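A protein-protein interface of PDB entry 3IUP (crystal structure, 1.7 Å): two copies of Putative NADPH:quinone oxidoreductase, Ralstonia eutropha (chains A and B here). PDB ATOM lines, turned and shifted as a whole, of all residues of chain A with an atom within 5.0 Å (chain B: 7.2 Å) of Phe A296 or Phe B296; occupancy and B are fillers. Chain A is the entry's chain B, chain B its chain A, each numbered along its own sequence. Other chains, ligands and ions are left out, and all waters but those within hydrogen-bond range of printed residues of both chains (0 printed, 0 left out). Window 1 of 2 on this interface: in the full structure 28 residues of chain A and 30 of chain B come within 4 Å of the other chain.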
ATOM      1  N   GLY A 255      19.889  13.106 -13.740  1.00  0.00           N
ATOM      2  CA  GLY A 255      18.559  13.420 -14.240  1.00  0.00           C
ATOM      3  C   GLY A 255      18.412  13.123 -15.713  1.00  0.00           C
ATOM      4  O   GLY A 255      17.334  12.713 -16.163  1.00  0.00           O
ATOM      5  N   PRO A 293      26.521  21.439  -8.028  1.00  0.00           N
ATOM      6  CA  PRO A 293      25.243  20.920  -7.554  1.00  0.00           C
ATOM      7  C   PRO A 293      24.619  19.891  -8.488  1.00  0.00           C
ATOM      8  O   PRO A 293      24.707  19.993  -9.721  1.00  0.00           O
ATOM      9  CB  PRO A 293      24.358  22.181  -7.469  1.00  0.00           C
ATOM     10  CG  PRO A 293      25.344  23.296  -7.252  1.00  0.00           C
ATOM     11  CD  PRO A 293      26.487  22.908  -8.163  1.00  0.00           C
ATOM     12  N   THR A 294      23.979  18.889  -7.908  1.00  0.00           N
ATOM     13  CA  THR A 294      23.075  18.020  -8.660  1.00  0.00           C
ATOM     14  C   THR A 294      21.843  18.805  -9.069  1.00  0.00           C
ATOM     15  O   THR A 294      21.265  19.515  -8.247  1.00  0.00           O
ATOM     16  CB  THR A 294      22.627  16.833  -7.803  1.00  0.00           C
ATOM     17  OG1 THR A 294      23.786  16.136  -7.346  1.00  0.00           O
ATOM     18  CG2 THR A 294      21.739  15.900  -8.552  1.00  0.00           C
ATOM     19  N   GLU A 295      21.434  18.689 -10.325  1.00  0.00           N
ATOM     20  CA  GLU A 295      20.310  19.454 -10.840  1.00  0.00           C
ATOM     21  C   GLU A 295      19.554  18.642 -11.859  1.00  0.00           C
ATOM     22  O   GLU A 295      20.172  17.990 -12.711  1.00  0.00           O
ATOM     23  CB  GLU A 295      20.865  20.748 -11.458  1.00  0.00           C
ATOM     24  CG  GLU A 295      19.855  21.633 -11.969  1.00  0.00           C
ATOM     25  CD  GLU A 295      20.466  22.862 -12.680  1.00  0.00           C
ATOM     26  OE1 GLU A 295      21.669  22.782 -13.117  1.00  0.00           O
ATOM     27  OE2 GLU A 295      19.709  23.877 -12.775  1.00  0.00           O
ATOM     28  N   PHE A 296      18.242  18.620 -11.761  1.00  0.00           N
ATOM     29  CA  PHE A 296      17.416  17.951 -12.759  1.00  0.00           C
ATOM     30  C   PHE A 296      15.974  18.435 -12.764  1.00  0.00           C
ATOM     31  O   PHE A 296      15.432  18.819 -11.714  1.00  0.00           O
ATOM     32  CB  PHE A 296      17.447  16.431 -12.575  1.00  0.00           C
ATOM     33  CG  PHE A 296      17.071  15.976 -11.183  1.00  0.00           C
ATOM     34  CD1 PHE A 296      15.743  15.692 -10.861  1.00  0.00           C
ATOM     35  CD2 PHE A 296      18.054  15.783 -10.207  1.00  0.00           C
ATOM     36  CE1 PHE A 296      15.398  15.270  -9.560  1.00  0.00           C
ATOM     37  CE2 PHE A 296      17.706  15.384  -8.895  1.00  0.00           C
ATOM     38  CZ  PHE A 296      16.398  15.137  -8.581  1.00  0.00           C
ATOM     39  N   ASN A 297      15.374  18.382 -13.949  1.00  0.00           N
ATOM     40  CA  ASN A 297      13.927  18.499 -14.097  1.00  0.00           C
ATOM     41  C   ASN A 297      13.271  17.154 -13.905  1.00  0.00           C
ATOM     42  O   ASN A 297      13.863  16.137 -14.154  1.00  0.00           O
ATOM     43  CB  ASN A 297      13.553  19.067 -15.449  1.00  0.00           C
ATOM     44  CG  ASN A 297      13.639  20.585 -15.461  1.00  0.00           C
ATOM     45  OD1 ASN A 297      13.071  21.274 -14.577  1.00  0.00           O
ATOM     46  ND2 ASN A 297      14.366  21.120 -16.440  1.00  0.00           N
ATOM     47  N   ARG A 298      12.039  17.164 -13.459  1.00  0.00           N
ATOM     48  CA  ARG A 298      11.356  15.974 -13.076  1.00  0.00           C
ATOM     49  C   ARG A 298      10.371  15.683 -14.170  1.00  0.00           C
ATOM     50  O   ARG A 298       9.173  15.988 -14.054  1.00  0.00           O
ATOM     51  CB  ARG A 298      10.688  16.181 -11.709  1.00  0.00           C
ATOM     52  CG  ARG A 298      11.730  16.319 -10.548  1.00  0.00           C
ATOM     53  CD  ARG A 298      11.046  16.787  -9.234  1.00  0.00           C
ATOM     54  NE  ARG A 298      10.184  17.923  -9.504  1.00  0.00           N
ATOM     55  CZ  ARG A 298      10.602  19.115  -9.881  1.00  0.00           C
ATOM     56  NH1 ARG A 298      11.883  19.374 -10.004  1.00  0.00           N
ATOM     57  NH2 ARG A 298       9.736  20.072 -10.179  1.00  0.00           N
ATOM     58  N   PHE A 300      10.031  12.625 -15.617  1.00  0.00           N
ATOM     59  CA  PHE A 300      10.113  11.186 -15.695  1.00  0.00           C
ATOM     60  C   PHE A 300       9.097  10.476 -14.826  1.00  0.00           C
ATOM     61  O   PHE A 300       9.249   9.305 -14.531  1.00  0.00           O
ATOM     62  CB  PHE A 300      11.551  10.705 -15.468  1.00  0.00           C
ATOM     63  CG  PHE A 300      12.281  11.438 -14.376  1.00  0.00           C
ATOM     64  CD1 PHE A 300      12.053  11.137 -13.084  1.00  0.00           C
ATOM     65  CD2 PHE A 300      13.228  12.395 -14.667  1.00  0.00           C
ATOM     66  CE1 PHE A 300      12.732  11.803 -12.075  1.00  0.00           C
ATOM     67  CE2 PHE A 300      13.915  13.003 -13.695  1.00  0.00           C
ATOM     68  CZ  PHE A 300      13.650  12.722 -12.375  1.00  0.00           C
ATOM     69  N   TRP A 304      10.582   6.693  -9.505  1.00  0.00           N
ATOM     70  CA  TRP A 304      12.027   6.903  -9.569  1.00  0.00           C
ATOM     71  C   TRP A 304      12.628   7.057  -8.186  1.00  0.00           C
ATOM     72  O   TRP A 304      11.926   7.429  -7.210  1.00  0.00           O
ATOM     73  CB  TRP A 304      12.331   8.150 -10.397  1.00  0.00           C
ATOM     74  CG  TRP A 304      11.878   9.441  -9.753  1.00  0.00           C
ATOM     75  CD1 TRP A 304      10.631   9.971  -9.787  1.00  0.00           C
ATOM     76  CD2 TRP A 304      12.659  10.308  -8.919  1.00  0.00           C
ATOM     77  NE1 TRP A 304      10.579  11.129  -9.047  1.00  0.00           N
ATOM     78  CE2 TRP A 304      11.817  11.365  -8.511  1.00  0.00           C
ATOM     79  CE3 TRP A 304      14.002  10.309  -8.507  1.00  0.00           C
ATOM     80  CZ2 TRP A 304      12.254  12.406  -7.718  1.00  0.00           C
ATOM     81  CZ3 TRP A 304      14.448  11.368  -7.691  1.00  0.00           C
ATOM     82  CH2 TRP A 304      13.575  12.402  -7.318  1.00  0.00           C
ATOM     83  N   MET A 306      16.766   8.151  -6.386  1.00  0.00           N
ATOM     84  CA  MET A 306      18.143   8.480  -6.495  1.00  0.00           C
ATOM     85  C   MET A 306      18.679   8.429  -5.081  1.00  0.00           C
ATOM     86  O   MET A 306      17.989   8.807  -4.126  1.00  0.00           O
ATOM     87  CB  MET A 306      18.297   9.903  -7.076  1.00  0.00           C
ATOM     88  CG  MET A 306      19.691  10.280  -7.452  1.00  0.00           C
ATOM     89  SD  MET A 306      19.723  12.204  -8.039  1.00  0.00           S
ATOM     90  CE  MET A 306      18.860  11.941  -9.824  1.00  0.00           C
ATOM     91  N   GLY B 249       8.978  19.652  -4.546  1.00  0.00           N
ATOM     92  CA  GLY B 249       9.610  18.869  -5.596  1.00  0.00           C
ATOM     93  C   GLY B 249      10.781  19.565  -6.255  1.00  0.00           C
ATOM     94  O   GLY B 249      11.964  19.182  -6.129  1.00  0.00           O
ATOM     95  N   GLY B 250      10.470  20.620  -7.008  1.00  0.00           N
ATOM     96  CA  GLY B 250      11.487  21.508  -7.457  1.00  0.00           C
ATOM     97  C   GLY B 250      12.205  22.309  -6.416  1.00  0.00           C
ATOM     98  O   GLY B 250      11.915  22.243  -5.214  1.00  0.00           O
ATOM     99  N   GLY B 251      13.172  23.082  -6.877  1.00  0.00           N
ATOM    100  CA  GLY B 251      13.940  23.918  -6.030  1.00  0.00           C
ATOM    101  C   GLY B 251      14.861  23.195  -5.058  1.00  0.00           C
ATOM    102  O   GLY B 251      15.359  22.101  -5.339  1.00  0.00           O
ATOM    103  N   LYS B 252      15.080  23.824  -3.918  1.00  0.00           N
ATOM    104  CA  LYS B 252      16.176  23.446  -3.053  1.00  0.00           C
ATOM    105  C   LYS B 252      15.799  22.758  -1.756  1.00  0.00           C
ATOM    106  O   LYS B 252      16.709  22.333  -1.020  1.00  0.00           O
ATOM    107  CB  LYS B 252      16.966  24.705  -2.700  1.00  0.00           C
ATOM    108  CG  LYS B 252      17.704  25.242  -3.901  1.00  0.00           C
ATOM    109  CD  LYS B 252      18.548  26.457  -3.496  1.00  0.00           C
ATOM    110  CE  LYS B 252      19.152  27.154  -4.700  1.00  0.00           C
ATOM    111  NZ  LYS B 252      20.198  28.136  -4.258  1.00  0.00           N
ATOM    112  N   LEU B 253      14.511  22.688  -1.455  1.00  0.00           N
ATOM    113  CA  LEU B 253      14.054  22.302  -0.129  1.00  0.00           C
ATOM    114  C   LEU B 253      14.446  20.851   0.221  1.00  0.00           C
ATOM    115  O   LEU B 253      14.882  20.565   1.325  1.00  0.00           O
ATOM    116  CB  LEU B 253      12.551  22.469  -0.008  1.00  0.00           C
ATOM    117  CG  LEU B 253      11.910  22.621   1.327  1.00  0.00           C
ATOM    118  CD1 LEU B 253      12.717  23.507   2.271  1.00  0.00           C
ATOM    119  CD2 LEU B 253      10.475  23.170   1.056  1.00  0.00           C
ATOM    120  N   GLY B 254      14.360  19.966  -0.764  1.00  0.00           N
ATOM    121  CA  GLY B 254      14.727  18.564  -0.493  1.00  0.00           C
ATOM    122  C   GLY B 254      16.160  18.427  -0.019  1.00  0.00           C
ATOM    123  O   GLY B 254      16.447  17.714   0.979  1.00  0.00           O
ATOM    124  N   GLY B 255      17.099  19.066  -0.726  1.00  0.00           N
ATOM    125  CA  GLY B 255      18.484  19.011  -0.339  1.00  0.00           C
ATOM    126  C   GLY B 255      18.784  19.735   0.964  1.00  0.00           C
ATOM    127  O   GLY B 255      19.608  19.291   1.778  1.00  0.00           O
ATOM    128  N   GLN B 256      18.106  20.871   1.158  1.00  0.00           N
ATOM    129  CA  GLN B 256      18.206  21.561   2.432  1.00  0.00           C
ATOM    130  C   GLN B 256      17.854  20.657   3.599  1.00  0.00           C
ATOM    131  O   GLN B 256      18.566  20.654   4.594  1.00  0.00           O
ATOM    132  CB  GLN B 256      17.365  22.798   2.425  1.00  0.00           C
ATOM    133  CG  GLN B 256      18.012  23.878   1.580  1.00  0.00           C
ATOM    134  CD  GLN B 256      17.102  25.061   1.337  1.00  0.00           C
ATOM    135  OE1 GLN B 256      15.892  24.939   1.348  1.00  0.00           O
ATOM    136  NE2 GLN B 256      17.704  26.194   1.012  1.00  0.00           N
ATOM    137  N   LEU B 258      17.892  17.323   3.705  1.00  0.00           N
ATOM    138  CA  LEU B 258      18.949  16.316   3.857  1.00  0.00           C
ATOM    139  C   LEU B 258      20.163  16.917   4.560  1.00  0.00           C
ATOM    140  O   LEU B 258      20.772  16.276   5.446  1.00  0.00           O
ATOM    141  CB  LEU B 258      19.325  15.715   2.508  1.00  0.00           C
ATOM    142  CG  LEU B 258      18.253  14.811   1.900  1.00  0.00           C
ATOM    143  CD1 LEU B 258      18.566  14.499   0.426  1.00  0.00           C
ATOM    144  CD2 LEU B 258      18.114  13.514   2.780  1.00  0.00           C
ATOM    145  N   THR B 259      20.572  18.097   4.137  1.00  0.00           N
ATOM    146  CA  THR B 259      21.730  18.750   4.733  1.00  0.00           C
ATOM    147  C   THR B 259      21.523  18.941   6.248  1.00  0.00           C
ATOM    148  O   THR B 259      22.421  18.652   7.066  1.00  0.00           O
ATOM    149  CB  THR B 259      22.027  20.094   3.988  1.00  0.00           C
ATOM    150  OG1 THR B 259      22.247  19.832   2.598  1.00  0.00           O
ATOM    151  CG2 THR B 259      23.230  20.846   4.568  1.00  0.00           C
ATOM    152  N   LEU B 285       9.533  13.083  -2.819  1.00  0.00           N
ATOM    153  CA  LEU B 285       8.938  14.213  -3.514  1.00  0.00           C
ATOM    154  C   LEU B 285       7.544  13.705  -3.905  1.00  0.00           C
ATOM    155  O   LEU B 285       7.395  12.986  -4.890  1.00  0.00           O
ATOM    156  CB  LEU B 285       9.756  14.621  -4.707  1.00  0.00           C
ATOM    157  CG  LEU B 285      11.223  14.944  -4.478  1.00  0.00           C
ATOM    158  CD1 LEU B 285      11.902  15.532  -5.752  1.00  0.00           C
ATOM    159  CD2 LEU B 285      11.455  15.827  -3.264  1.00  0.00           C
ATOM    160  N   SER B 292      10.196  24.360 -10.914  1.00  0.00           N
ATOM    161  CA  SER B 292      11.592  24.553 -11.322  1.00  0.00           C
ATOM    162  C   SER B 292      12.428  23.246 -11.144  1.00  0.00           C
ATOM    163  O   SER B 292      11.954  22.327 -10.495  1.00  0.00           O
ATOM    164  CB  SER B 292      12.270  25.645 -10.505  1.00  0.00           C
ATOM    165  OG  SER B 292      12.534  25.281  -9.162  1.00  0.00           O
ATOM    166  N   PRO B 293      13.620  23.205 -11.764  1.00  0.00           N
ATOM    167  CA  PRO B 293      14.532  22.061 -11.523  1.00  0.00           C
ATOM    168  C   PRO B 293      14.823  21.860 -10.039  1.00  0.00           C
ATOM    169  O   PRO B 293      14.961  22.827  -9.244  1.00  0.00           O
ATOM    170  CB  PRO B 293      15.827  22.472 -12.191  1.00  0.00           C
ATOM    171  CG  PRO B 293      15.428  23.573 -13.222  1.00  0.00           C
ATOM    172  CD  PRO B 293      14.278  24.279 -12.524  1.00  0.00           C
ATOM    173  N   THR B 294      14.952  20.590  -9.685  1.00  0.00           N
ATOM    174  CA  THR B 294      15.420  20.191  -8.371  1.00  0.00           C
ATOM    175  C   THR B 294      16.922  20.412  -8.362  1.00  0.00           C
ATOM    176  O   THR B 294      17.626  20.028  -9.319  1.00  0.00           O
ATOM    177  CB  THR B 294      15.081  18.698  -8.093  1.00  0.00           C
ATOM    178  OG1 THR B 294      13.662  18.482  -8.116  1.00  0.00           O
ATOM    179  CG2 THR B 294      15.684  18.254  -6.730  1.00  0.00           C
ATOM    180  N   GLU B 295      17.431  21.037  -7.309  1.00  0.00           N
ATOM    181  CA  GLU B 295      18.839  21.355  -7.179  1.00  0.00           C
ATOM    182  C   GLU B 295      19.343  21.161  -5.761  1.00  0.00           C
ATOM    183  O   GLU B 295      18.758  21.653  -4.818  1.00  0.00           O
ATOM    184  CB  GLU B 295      19.097  22.833  -7.574  1.00  0.00           C
ATOM    185  CG  GLU B 295      20.588  23.180  -7.703  1.00  0.00           C
ATOM    186  CD  GLU B 295      20.892  24.692  -7.837  1.00  0.00           C
ATOM    187  OE1 GLU B 295      19.975  25.528  -7.667  1.00  0.00           O
ATOM    188  OE2 GLU B 295      22.074  25.024  -8.071  1.00  0.00           O
ATOM    189  N   PHE B 296      20.468  20.479  -5.596  1.00  0.00           N
ATOM    190  CA  PHE B 296      21.066  20.354  -4.277  1.00  0.00           C
ATOM    191  C   PHE B 296      22.556  20.072  -4.320  1.00  0.00           C
ATOM    192  O   PHE B 296      23.017  19.447  -5.267  1.00  0.00           O
ATOM    193  CB  PHE B 296      20.364  19.283  -3.447  1.00  0.00           C
ATOM    194  CG  PHE B 296      20.279  17.918  -4.104  1.00  0.00           C
ATOM    195  CD1 PHE B 296      21.263  16.972  -3.891  1.00  0.00           C
ATOM    196  CD2 PHE B 296      19.187  17.568  -4.885  1.00  0.00           C
ATOM    197  CE1 PHE B 296      21.154  15.690  -4.466  1.00  0.00           C
ATOM    198  CE2 PHE B 296      19.051  16.290  -5.431  1.00  0.00           C
ATOM    199  CZ  PHE B 296      20.061  15.361  -5.234  1.00  0.00           C
ATOM    200  N   ASN B 297      23.278  20.565  -3.312  1.00  0.00           N
ATOM    201  CA  ASN B 297      24.649  20.159  -3.021  1.00  0.00           C
ATOM    202  C   ASN B 297      24.639  18.917  -2.170  1.00  0.00           C
ATOM    203  O   ASN B 297      23.769  18.752  -1.402  1.00  0.00           O
ATOM    204  CB  ASN B 297      25.399  21.254  -2.310  1.00  0.00           C
ATOM    205  CG  ASN B 297      25.886  22.265  -3.298  1.00  0.00           C
ATOM    206  OD1 ASN B 297      26.442  21.875  -4.327  1.00  0.00           O
ATOM    207  ND2 ASN B 297      25.590  23.534  -3.060  1.00  0.00           N
ATOM    208  N   ARG B 298      25.583  18.037  -2.360  1.00  0.00           N
ATOM    209  CA  ARG B 298      25.512  16.766  -1.676  1.00  0.00           C
ATOM    210  C   ARG B 298      26.377  16.781  -0.431  1.00  0.00           C
ATOM    211  O   ARG B 298      27.320  15.999  -0.336  1.00  0.00           O
ATOM    212  CB  ARG B 298      25.987  15.688  -2.636  1.00  0.00           C
ATOM    213  CG  ARG B 298      24.986  15.461  -3.762  1.00  0.00           C
ATOM    214  CD  ARG B 298      25.582  14.616  -4.930  1.00  0.00           C
ATOM    215  NE  ARG B 298      26.861  15.143  -5.355  1.00  0.00           N
ATOM    216  CZ  ARG B 298      27.038  16.287  -6.009  1.00  0.00           C
ATOM    217  NH1 ARG B 298      26.006  17.039  -6.341  1.00  0.00           N
ATOM    218  NH2 ARG B 298      28.250  16.719  -6.283  1.00  0.00           N
ATOM    219  N   ASN B 299      26.066  17.611   0.541  1.00  0.00           N
ATOM    220  CA  ASN B 299      26.915  17.761   1.710  1.00  0.00           C
ATOM    221  C   ASN B 299      26.308  17.012   2.891  1.00  0.00           C
ATOM    222  O   ASN B 299      26.294  17.520   4.014  1.00  0.00           O
ATOM    223  CB  ASN B 299      27.105  19.266   2.006  1.00  0.00           C
ATOM    224  CG  ASN B 299      25.815  20.044   1.877  1.00  0.00           C
ATOM    225  OD1 ASN B 299      24.736  19.450   1.759  1.00  0.00           O
ATOM    226  ND2 ASN B 299      25.909  21.372   1.869  1.00  0.00           N
ATOM    227  N   PHE B 300      25.788  15.811   2.635  1.00  0.00           N
ATOM    228  CA  PHE B 300      25.096  15.057   3.634  1.00  0.00           C
ATOM    229  C   PHE B 300      25.478  13.575   3.629  1.00  0.00           C
ATOM    230  O   PHE B 300      24.773  12.733   4.143  1.00  0.00           O
ATOM    231  CB  PHE B 300      23.582  15.297   3.490  1.00  0.00           C
ATOM    232  CG  PHE B 300      23.065  15.277   2.059  1.00  0.00           C
ATOM    233  CD1 PHE B 300      22.986  14.096   1.340  1.00  0.00           C
ATOM    234  CD2 PHE B 300      22.642  16.446   1.428  1.00  0.00           C
ATOM    235  CE1 PHE B 300      22.489  14.101   0.023  1.00  0.00           C
ATOM    236  CE2 PHE B 300      22.163  16.437   0.145  1.00  0.00           C
ATOM    237  CZ  PHE B 300      22.083  15.275  -0.563  1.00  0.00           C
ATOM    238  N   TRP B 304      21.562   8.321   2.014  1.00  0.00           N
ATOM    239  CA  TRP B 304      20.429   9.136   1.672  1.00  0.00           C
ATOM    240  C   TRP B 304      19.735   8.598   0.449  1.00  0.00           C
ATOM    241  O   TRP B 304      20.344   7.900  -0.386  1.00  0.00           O
ATOM    242  CB  TRP B 304      20.858  10.609   1.409  1.00  0.00           C
ATOM    243  CG  TRP B 304      21.707  10.784   0.189  1.00  0.00           C
ATOM    244  CD1 TRP B 304      23.034  10.632   0.108  1.00  0.00           C
ATOM    245  CD2 TRP B 304      21.252  11.116  -1.149  1.00  0.00           C
ATOM    246  NE1 TRP B 304      23.451  10.793  -1.183  1.00  0.00           N
ATOM    247  CE2 TRP B 304      22.387  11.109  -1.979  1.00  0.00           C
ATOM    248  CE3 TRP B 304      20.002  11.417  -1.704  1.00  0.00           C
ATOM    249  CZ2 TRP B 304      22.333  11.407  -3.333  1.00  0.00           C
ATOM    250  CZ3 TRP B 304      19.936  11.696  -3.051  1.00  0.00           C
ATOM    251  CH2 TRP B 304      21.100  11.717  -3.852  1.00  0.00           C
ATOM    252  N   MET B 306      16.269   9.883  -2.295  1.00  0.00           N
ATOM    253  CA  MET B 306      15.244  10.839  -2.682  1.00  0.00           C
ATOM    254  C   MET B 306      14.434  10.125  -3.751  1.00  0.00           C
ATOM    255  O   MET B 306      15.006   9.423  -4.624  1.00  0.00           O
ATOM    256  CB  MET B 306      15.853  12.113  -3.282  1.00  0.00           C
ATOM    257  CG  MET B 306      14.818  13.147  -3.575  1.00  0.00           C
ATOM    258  SD  MET B 306      15.713  14.790  -4.330  1.00  0.00           S
ATOM    259  CE  MET B 306      16.742  15.406  -2.771  1.00  0.00           C
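Hydrophobic or aromatic side chains of chain B within 4 Å of the printed part of chain A: Leu B285, Pro B293, Phe B296 and Trp B304.
Printed residues of chain A that touch a printed residue of chain B: Pro A293, Thr A294, Glu A295, Phe A296, Asn A297, Arg A298, Trp A304 and Met A306.
Hydrophobic or aromatic side chains of chain A that line the printed part of chain B: Pro A293, Phe A296 and Trp A304.
Along chain A the printed residues that touch a printed residue of chain B span positions 293 to 306.
Among the printed residues, 23 pairs touch across the chains.
Among the printed residues, no Asp or Glu carboxylate lies within 4 Å of a Lys or Arg side-chain nitrogen of the other chain.
The side-chain hydroxyl (OG1) of Thr B294 sits at hydrogen-bond distance from the guanidinium group (NH1) of Arg A298, 2.7 Å away.
The backbone carbonyl oxygen (O) of Phe B296 is in hydrogen-bond range of the backbone NH (N) of Thr A294.
The side-chain amide oxygen of Asn A297 sits close to the backbone nitrogen of Pro B293, at 3.5 Å.
The guanidinium group (NH1) of Arg B298 lies within hydrogen-bond range of the side-chain hydroxyl (OG1) of Thr A294 (2.6 Å).
N of Met B306 is in hydrogen-bond range of O of Met A306 (2.7 Å).
The backbone carbonyl oxygen (O) of Phe A296 is in hydrogen-bond range of the backbone NH (N) of Thr B294, 2.7 Å away.
The guanidinium group (NH2) of Arg A298 sits close to the backbone NH (N) of Gly B250 (3.3 Å).
NH1 of Arg A298 is in hydrogen-bond range of O of Ser B292 (3.0 Å).
Pro A293 touches Glu B295, but with the chains exchanged Glu A295 does not touch Pro B293 (4.1 Å).
Pro A293 touches Phe B296, and with the chains exchanged Phe A296 touches Pro B293.
Thr A294 touches its own counterpart, Thr B294.
Met A306 touches its own counterpart, Met B306.
Of the 23 pairs that touch across the chains among the printed residues, 17 have their exchanged pair printed and touching as well.
The side-chain amide oxygen of Asn B299 lies close to the backbone carbonyl oxygen of Asn B297, 3.4 Å away.
The backbone carbonyl oxygen (O) of Gly B249 sits at hydrogen-bond distance from the side-chain hydroxyl (OG1) of Thr B294, 2.7 Å away.
N of Glu B295 lies within hydrogen-bond range of O of Gly B251, at 3.1 Å.
The backbone NH (N) of Gly B251 is in hydrogen-bond range of the side-chain hydroxyl (OG) of Ser B292, at 3.2 Å.
N of Gly B251 is in hydrogen-bond range of O of Pro B293, at 3.0 Å.
Among the printed residues, pairs that only touch across the chains: Pro A293 with Glu B295 (3.7 Å), Pro A293 with Phe B296 (3.5 Å), Pro A293 with Asn B297 (3.4 Å), Pro A293 with Arg B298 (3.8 Å), Thr A294 with Thr B294 (3.8 Å), Thr A294 with Glu B295 (3.2 Å), Glu A295 with Thr B294 (3.1 Å), Phe A296 with Pro B293 (3.4 Å), Phe A296 with Phe B296 (3.8 Å), Arg A298 with Gly B249 (3.7 Å), Arg A298 with Leu B285 (3.8 Å), Arg A298 with Pro B293 (3.9 Å), Trp A304 with Leu B285 (3.7 Å), Trp A304 with Met B306 (3.7 Å) and Met A306 with Trp B304 (3.6 Å).
Of the printed residues of chain B, Pro A293 touches Glu B295 (3.7 Å), Phe B296 (3.5 Å), Asn B297 (3.4 Å) and Arg B298 (3.8 Å).
Of chain B, only Pro B293 (3.4 Å), Thr B294 (2.7 Å) and Phe B296 (3.8 Å) come within 4 Å of Phe A296.
Printed residues of chain B within 4 Å of Met A306: Trp B304 (3.6 Å) and Met B306 (2.7 Å).
Gly B254 touches none of the printed residues of chain A.
Of the printed residues of chain A, Pro B293 touches Phe A296 (3.4 Å), Asn A297 (3.5 Å) and Arg A298 (3.9 Å).
Of the printed residues of chain A, Glu B295 touches Pro A293 and Thr A294.
The nearest residue of chain B that does not touch Phe A296 is Met B306 (4.3 Å).
The nearest residue of chain A that does not touch Phe B296 is Met A306 (4.2 Å).
The nearest printed residue of chain B that does not touch Met A306 is Phe B296 (4.2 Å).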
